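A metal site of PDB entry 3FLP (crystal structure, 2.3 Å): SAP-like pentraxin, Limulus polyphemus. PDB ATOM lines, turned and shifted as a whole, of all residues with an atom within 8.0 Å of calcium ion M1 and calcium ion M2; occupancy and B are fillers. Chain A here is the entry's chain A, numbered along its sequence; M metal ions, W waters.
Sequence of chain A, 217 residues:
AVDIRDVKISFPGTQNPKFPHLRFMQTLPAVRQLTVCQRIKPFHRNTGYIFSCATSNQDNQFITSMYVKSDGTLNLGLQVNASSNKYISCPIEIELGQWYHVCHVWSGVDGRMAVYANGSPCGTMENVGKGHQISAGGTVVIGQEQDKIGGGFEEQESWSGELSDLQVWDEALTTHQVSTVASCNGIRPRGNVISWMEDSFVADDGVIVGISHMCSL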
ATOM      1  N   TYR A  49      14.714  -7.620  20.772  1.00  0.00           N
ATOM      2  CA  TYR A  49      15.499  -7.056  19.669  1.00  0.00           C
ATOM      3  C   TYR A  49      16.647  -6.239  20.224  1.00  0.00           C
ATOM      4  O   TYR A  49      16.457  -5.351  21.058  1.00  0.00           O
ATOM      5  CB  TYR A  49      14.600  -6.193  18.777  1.00  0.00           C
ATOM      6  CG  TYR A  49      13.586  -7.031  18.044  1.00  0.00           C
ATOM      7  CD1 TYR A  49      12.450  -7.509  18.696  1.00  0.00           C
ATOM      8  CD2 TYR A  49      13.807  -7.436  16.727  1.00  0.00           C
ATOM      9  CE1 TYR A  49      11.569  -8.374  18.070  1.00  0.00           C
ATOM     10  CE2 TYR A  49      12.941  -8.311  16.084  1.00  0.00           C
ATOM     11  CZ  TYR A  49      11.822  -8.775  16.757  1.00  0.00           C
ATOM     12  OH  TYR A  49      10.972  -9.647  16.132  1.00  0.00           O
ATOM     13  N   SER A  52      18.552  -2.327  16.268  1.00  0.00           N
ATOM     14  CA  SER A  52      17.458  -1.878  15.409  1.00  0.00           C
ATOM     15  C   SER A  52      17.857  -0.676  14.554  1.00  0.00           C
ATOM     16  O   SER A  52      18.271   0.352  15.086  1.00  0.00           O
ATOM     17  CB  SER A  52      16.236  -1.519  16.271  1.00  0.00           C
ATOM     18  OG  SER A  52      15.250  -0.807  15.546  1.00  0.00           O
ATOM     19  N   CYS A  53      17.745  -0.816  13.230  1.00  0.00           N
ATOM     20  CA  CYS A  53      18.084   0.257  12.305  1.00  0.00           C
ATOM     21  C   CYS A  53      16.851   0.661  11.493  1.00  0.00           C
ATOM     22  O   CYS A  53      16.207  -0.179  10.875  1.00  0.00           O
ATOM     23  CB  CYS A  53      19.199  -0.180  11.366  1.00  0.00           C
ATOM     24  SG  CYS A  53      19.676   1.112  10.195  1.00  0.00           S
ATOM     25  N   ALA A  54      16.546   1.957  11.491  1.00  0.00           N
ATOM     26  CA  ALA A  54      15.374   2.444  10.779  1.00  0.00           C
ATOM     27  C   ALA A  54      15.615   3.712   9.960  1.00  0.00           C
ATOM     28  O   ALA A  54      16.372   4.581  10.375  1.00  0.00           O
ATOM     29  CB  ALA A  54      14.245   2.677  11.766  1.00  0.00           C
ATOM     30  N   GLN A  58      11.362   3.132   6.122  1.00  0.00           N
ATOM     31  CA  GLN A  58      11.419   1.738   6.545  1.00  0.00           C
ATOM     32  C   GLN A  58      11.951   1.590   7.964  1.00  0.00           C
ATOM     33  O   GLN A  58      13.157   1.631   8.184  1.00  0.00           O
ATOM     34  CB  GLN A  58      12.320   0.955   5.575  1.00  0.00           C
ATOM     35  CG  GLN A  58      12.528  -0.523   5.906  1.00  0.00           C
ATOM     36  CD  GLN A  58      11.222  -1.273   6.109  1.00  0.00           C
ATOM     37  OE1 GLN A  58      10.688  -1.303   7.207  1.00  0.00           O
ATOM     38  NE2 GLN A  58      10.700  -1.847   5.027  1.00  0.00           N
ATOM     39  N   ASP A  59      11.040   1.412   8.921  1.00  0.00           N
ATOM     40  CA  ASP A  59      11.449   1.273  10.310  1.00  0.00           C
ATOM     41  C   ASP A  59      12.160  -0.045  10.594  1.00  0.00           C
ATOM     42  O   ASP A  59      12.802  -0.191  11.635  1.00  0.00           O
ATOM     43  CB  ASP A  59      10.229   1.432  11.239  1.00  0.00           C
ATOM     44  CG  ASP A  59       9.158   0.366  11.026  1.00  0.00           C
ATOM     45  OD1 ASP A  59       8.719   0.162   9.877  1.00  0.00           O
ATOM     46  OD2 ASP A  59       8.735  -0.260  12.031  1.00  0.00           O
ATOM     47  N   ASN A  60      12.050  -0.990   9.664  1.00  0.00           N
ATOM     48  CA  ASN A  60      12.667  -2.299   9.836  1.00  0.00           C
ATOM     49  C   ASN A  60      13.759  -2.607   8.797  1.00  0.00           C
ATOM     50  O   ASN A  60      13.727  -3.642   8.132  1.00  0.00           O
ATOM     51  CB  ASN A  60      11.576  -3.382   9.784  1.00  0.00           C
ATOM     52  CG  ASN A  60      10.626  -3.311  10.993  1.00  0.00           C
ATOM     53  OD1 ASN A  60      10.549  -2.291  11.682  1.00  0.00           O
ATOM     54  ND2 ASN A  60       9.896  -4.401  11.238  1.00  0.00           N
ATOM     55  N   GLN A  61      14.717  -1.699   8.659  1.00  0.00           N
ATOM     56  CA  GLN A  61      15.806  -1.887   7.693  1.00  0.00           C
ATOM     57  C   GLN A  61      16.710  -3.063   8.069  1.00  0.00           C
ATOM     58  O   GLN A  61      17.053  -3.886   7.222  1.00  0.00           O
ATOM     59  CB  GLN A  61      16.638  -0.608   7.596  1.00  0.00           C
ATOM     60  CG  GLN A  61      16.024   0.467   6.716  1.00  0.00           C
ATOM     61  CD  GLN A  61      16.211   0.186   5.227  1.00  0.00           C
ATOM     62  OE1 GLN A  61      16.605  -0.913   4.829  1.00  0.00           O
ATOM     63  NE2 GLN A  61      15.938   1.184   4.399  1.00  0.00           N
ATOM     64  N   ILE A  63      17.311  -5.587  11.704  1.00  0.00           N
ATOM     65  CA  ILE A  63      17.054  -5.820  13.125  1.00  0.00           C
ATOM     66  C   ILE A  63      17.532  -7.187  13.574  1.00  0.00           C
ATOM     67  O   ILE A  63      17.194  -8.217  12.979  1.00  0.00           O
ATOM     68  CB  ILE A  63      15.547  -5.726  13.464  1.00  0.00           C
ATOM     69  CG1 ILE A  63      14.781  -5.047  12.322  1.00  0.00           C
ATOM     70  CG2 ILE A  63      15.371  -4.918  14.742  1.00  0.00           C
ATOM     71  CD1 ILE A  63      13.282  -5.013  12.537  1.00  0.00           C
ATOM     72  N   GLN A  79      16.321  -9.687  10.584  1.00  0.00           N
ATOM     73  CA  GLN A  79      15.262  -9.214   9.722  1.00  0.00           C
ATOM     74  C   GLN A  79      15.862  -8.079   8.905  1.00  0.00           C
ATOM     75  O   GLN A  79      16.512  -7.193   9.447  1.00  0.00           O
ATOM     76  CB  GLN A  79      14.058  -8.726  10.549  1.00  0.00           C
ATOM     77  CG  GLN A  79      13.044  -7.939   9.732  1.00  0.00           C
ATOM     78  CD  GLN A  79      11.749  -7.624  10.475  1.00  0.00           C
ATOM     79  OE1 GLN A  79      10.998  -6.732  10.073  1.00  0.00           O
ATOM     80  NE2 GLN A  79      11.474  -8.374  11.538  1.00  0.00           N
ATOM     81  N   GLN A 144      15.682  -1.700  22.001  1.00  0.00           N
ATOM     82  CA  GLN A 144      14.272  -1.544  21.671  1.00  0.00           C
ATOM     83  C   GLN A 144      14.104  -1.687  20.159  1.00  0.00           C
ATOM     84  O   GLN A 144      15.062  -1.529  19.409  1.00  0.00           O
ATOM     85  CB  GLN A 144      13.740  -0.166  22.110  1.00  0.00           C
ATOM     86  CG  GLN A 144      13.847   0.180  23.604  1.00  0.00           C
ATOM     87  CD  GLN A 144      12.977  -0.710  24.499  1.00  0.00           C
ATOM     88  OE1 GLN A 144      11.974  -1.268  24.066  1.00  0.00           O
ATOM     89  NE2 GLN A 144      13.361  -0.817  25.754  1.00  0.00           N
ATOM     90  N   GLU A 145      12.881  -1.993  19.719  1.00  0.00           N
ATOM     91  CA  GLU A 145      12.560  -2.157  18.305  1.00  0.00           C
ATOM     92  C   GLU A 145      11.847  -0.878  17.852  1.00  0.00           C
ATOM     93  O   GLU A 145      10.813  -0.518  18.422  1.00  0.00           O
ATOM     94  CB  GLU A 145      11.642  -3.379  18.152  1.00  0.00           C
ATOM     95  CG  GLU A 145      11.681  -4.081  16.787  1.00  0.00           C
ATOM     96  CD  GLU A 145      10.940  -3.334  15.698  1.00  0.00           C
ATOM     97  OE1 GLU A 145       9.741  -3.003  15.899  1.00  0.00           O
ATOM     98  OE2 GLU A 145      11.550  -3.067  14.640  1.00  0.00           O
ATOM     99  N   GLN A 146      12.387  -0.183  16.856  1.00  0.00           N
ATOM    100  CA  GLN A 146      11.781   1.053  16.354  1.00  0.00           C
ATOM    101  C   GLN A 146      10.625   0.841  15.378  1.00  0.00           C
ATOM    102  O   GLN A 146      10.708   0.007  14.479  1.00  0.00           O
ATOM    103  CB  GLN A 146      12.814   1.918  15.634  1.00  0.00           C
ATOM    104  CG  GLN A 146      14.047   2.318  16.425  1.00  0.00           C
ATOM    105  CD  GLN A 146      15.113   2.950  15.532  1.00  0.00           C
ATOM    106  OE1 GLN A 146      15.055   4.138  15.206  1.00  0.00           O
ATOM    107  NE2 GLN A 146      16.092   2.142  15.130  1.00  0.00           N
ATOM    108  N   ASP A 147       9.535   1.598  15.572  1.00  0.00           N
ATOM    109  CA  ASP A 147       8.392   1.557  14.667  1.00  0.00           C
ATOM    110  C   ASP A 147       8.331   2.932  14.028  1.00  0.00           C
ATOM    111  O   ASP A 147       7.508   3.214  13.163  1.00  0.00           O
ATOM    112  CB  ASP A 147       7.094   1.238  15.412  1.00  0.00           C
ATOM    113  CG  ASP A 147       6.969  -0.227  15.748  1.00  0.00           C
ATOM    114  OD1 ASP A 147       7.566  -1.050  15.016  1.00  0.00           O
ATOM    115  OD2 ASP A 147       6.259  -0.571  16.716  1.00  0.00           O
ATOM    116  N   LYS A 148       9.247   3.781  14.492  1.00  0.00           N
ATOM    117  CA  LYS A 148       9.415   5.145  13.993  1.00  0.00           C
ATOM    118  C   LYS A 148      10.845   5.507  14.362  1.00  0.00           C
ATOM    119  O   LYS A 148      11.434   4.901  15.259  1.00  0.00           O
ATOM    120  CB  LYS A 148       8.441   6.118  14.657  1.00  0.00           C
ATOM    121  CG  LYS A 148       8.589   6.193  16.168  1.00  0.00           C
ATOM    122  CD  LYS A 148       8.090   7.516  16.745  1.00  0.00           C
ATOM    123  CE  LYS A 148       6.612   7.747  16.472  1.00  0.00           C
ATOM    124  NZ  LYS A 148       6.139   8.952  17.193  1.00  0.00           N
ATOM    125  N   GLY A 151      11.867   5.827  18.056  1.00  0.00           N
ATOM    126  CA  GLY A 151      10.734   5.645  18.941  1.00  0.00           C
ATOM    127  C   GLY A 151       9.742   4.571  18.536  1.00  0.00           C
ATOM    128  O   GLY A 151      10.077   3.660  17.775  1.00  0.00           O
ATOM    129  N   GLY A 152       8.519   4.690  19.041  1.00  0.00           N
ATOM    130  CA  GLY A 152       7.469   3.718  18.751  1.00  0.00           C
ATOM    131  C   GLY A 152       7.836   2.360  19.316  1.00  0.00           C
ATOM    132  O   GLY A 152       7.541   1.332  18.721  1.00  0.00           O
ATOM    133  N   PHE A 153       8.472   2.367  20.481  1.00  0.00           N
ATOM    134  CA  PHE A 153       8.908   1.141  21.146  1.00  0.00           C
ATOM    135  C   PHE A 153       7.745   0.331  21.722  1.00  0.00           C
ATOM    136  O   PHE A 153       6.706   0.869  22.083  1.00  0.00           O
ATOM    137  CB  PHE A 153       9.884   1.461  22.281  1.00  0.00           C
ATOM    138  CG  PHE A 153      11.071   2.289  21.852  1.00  0.00           C
ATOM    139  CD1 PHE A 153      11.714   2.028  20.653  1.00  0.00           C
ATOM    140  CD2 PHE A 153      11.533   3.315  22.658  1.00  0.00           C
ATOM    141  CE1 PHE A 153      12.816   2.794  20.252  1.00  0.00           C
ATOM    142  CE2 PHE A 153      12.642   4.087  22.277  1.00  0.00           C
ATOM    143  CZ  PHE A 153      13.281   3.818  21.068  1.00  0.00           C
ATOM    144  N   GLU A 154       7.949  -0.985  21.819  1.00  0.00           N
ATOM    145  CA  GLU A 154       6.950  -1.903  22.358  1.00  0.00           C
ATOM    146  C   GLU A 154       7.619  -2.809  23.382  1.00  0.00           C
ATOM    147  O   GLU A 154       8.628  -3.456  23.077  1.00  0.00           O
ATOM    148  CB  GLU A 154       6.335  -2.752  21.231  1.00  0.00           C
ATOM    149  CG  GLU A 154       5.463  -1.956  20.285  1.00  0.00           C
ATOM    150  CD  GLU A 154       4.883  -2.804  19.171  1.00  0.00           C
ATOM    151  OE1 GLU A 154       5.642  -3.195  18.250  1.00  0.00           O
ATOM    152  OE2 GLU A 154       3.669  -3.082  19.213  1.00  0.00           O
ATOM    153  N   GLU A 155       7.057  -2.864  24.576  1.00  0.00           N
ATOM    154  CA  GLU A 155       7.648  -3.671  25.646  1.00  0.00           C
ATOM    155  C   GLU A 155       7.873  -5.145  25.315  1.00  0.00           C
ATOM    156  O   GLU A 155       8.857  -5.727  25.755  1.00  0.00           O
ATOM    157  CB  GLU A 155       6.840  -3.521  26.944  1.00  0.00           C
ATOM    158  CG  GLU A 155       5.342  -3.776  26.832  1.00  0.00           C
ATOM    159  CD  GLU A 155       4.599  -3.497  28.146  1.00  0.00           C
ATOM    160  OE1 GLU A 155       4.679  -2.349  28.667  1.00  0.00           O
ATOM    161  OE2 GLU A 155       3.917  -4.419  28.655  1.00  0.00           O
ATOM    162  N   GLN A 156       6.973  -5.747  24.537  1.00  0.00           N
ATOM    163  CA  GLN A 156       7.141  -7.155  24.195  1.00  0.00           C
ATOM    164  C   GLN A 156       8.272  -7.428  23.197  1.00  0.00           C
ATOM    165  O   GLN A 156       8.606  -8.575  22.941  1.00  0.00           O
ATOM    166  CB  GLN A 156       5.825  -7.739  23.677  1.00  0.00           C
ATOM    167  CG  GLN A 156       4.787  -7.943  24.787  1.00  0.00           C
ATOM    168  CD  GLN A 156       3.553  -8.694  24.301  1.00  0.00           C
ATOM    169  OE1 GLN A 156       2.817  -8.208  23.423  1.00  0.00           O
ATOM    170  NE2 GLN A 156       3.307  -9.871  24.878  1.00  0.00           N
ATOM    171  N   GLU A 157       8.863  -6.374  22.638  1.00  0.00           N
ATOM    172  CA  GLU A 157       9.961  -6.547  21.694  1.00  0.00           C
ATOM    173  C   GLU A 157      11.280  -6.002  22.244  1.00  0.00           C
ATOM    174  O   GLU A 157      12.305  -6.002  21.544  1.00  0.00           O
ATOM    175  CB  GLU A 157       9.614  -5.872  20.369  1.00  0.00           C
ATOM    176  CG  GLU A 157       8.370  -6.461  19.704  1.00  0.00           C
ATOM    177  CD  GLU A 157       7.972  -5.724  18.429  1.00  0.00           C
ATOM    178  OE1 GLU A 157       7.920  -4.484  18.455  1.00  0.00           O
ATOM    179  OE2 GLU A 157       7.687  -6.390  17.412  1.00  0.00           O
HETATM  180 CA    CA M   1       7.490  -2.664  16.991  1.00  0.00          CA
HETATM  181 CA    CA M   2       9.434  -1.850  13.696  1.00  0.00          CA
HETATM  182  O   HOH W   1       8.359  -1.239  18.674  1.00  0.00           O
HETATM  183  O   HOH W   2       8.020  -3.714  13.553  1.00  0.00           O
HETATM  184  O   HOH W   3       6.881  -4.569  15.737  1.00  0.00           O
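Calcium ion M1 is bound by the side-chain carboxylate (OE1) of Glu 154, at 2.3 Å. Water W3 binds calcium ion M1 (2.4 Å). Water W1 is bound to calcium ion M1, at 2.4 Å. OE1 of Glu 157 is bound to calcium ion M1, 2.4 Å away. The side-chain carboxylate (OD2) of Asp 147 is bound to calcium ion M1 (2.4 Å). The side-chain carboxylate (OE1) of Glu 145 binds calcium ion M1, at 2.5 Å. OD1 of Asp 147 is bound to calcium ion M1, 2.6 Å away. Calcium ion M1 has seven donor atoms within binding distance.
Calcium ion M2 is bound by the side-chain amide oxygen (OD1) of Asn 60 (2.3 Å), water W2 (2.3 Å), the backbone carbonyl oxygen (O) of Gln 146 (2.4 Å), the side-chain carboxylate (OD2) of Asp 59 (2.4 Å), the side-chain carboxylate (OD1) of Asp 147 (2.4 Å), the side-chain carboxylate (OE1) of Glu 145 (2.5 Å) and the side-chain carboxylate (OE2) of Glu 145 (2.6 Å).
Water W1 lies within hydrogen-bond range of O of Glu 145 (2.6 Å), O of Gly 152 (2.7 Å) and N of Glu 154 (3.2 Å).
Within 4 Å of calcium ion M2: Asp 59, Asn 60, Glu 145, Gln 146 and Asp 147.
The backbone NH of Asn 60 is in hydrogen-bond range of the side-chain amide oxygen of Gln 58. O of Glu 157 sits at hydrogen-bond distance from N of Tyr 49 (3.0 Å). The backbone carbonyl oxygen of Ser 52 sits at hydrogen-bond distance from the side-chain amide nitrogen of Gln 146. The side-chain amide nitrogen (ND2) of Asn 60 lies within hydrogen-bond range of the side-chain amide oxygen (OE1) of Gln 79, at 2.8 Å.
Within 4 Å of calcium ion M1: Glu 145, Asp 147, Glu 154 and Glu 157. Along chain A the residues within 4 Å of calcium ion M1 span positions 145 to 157.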
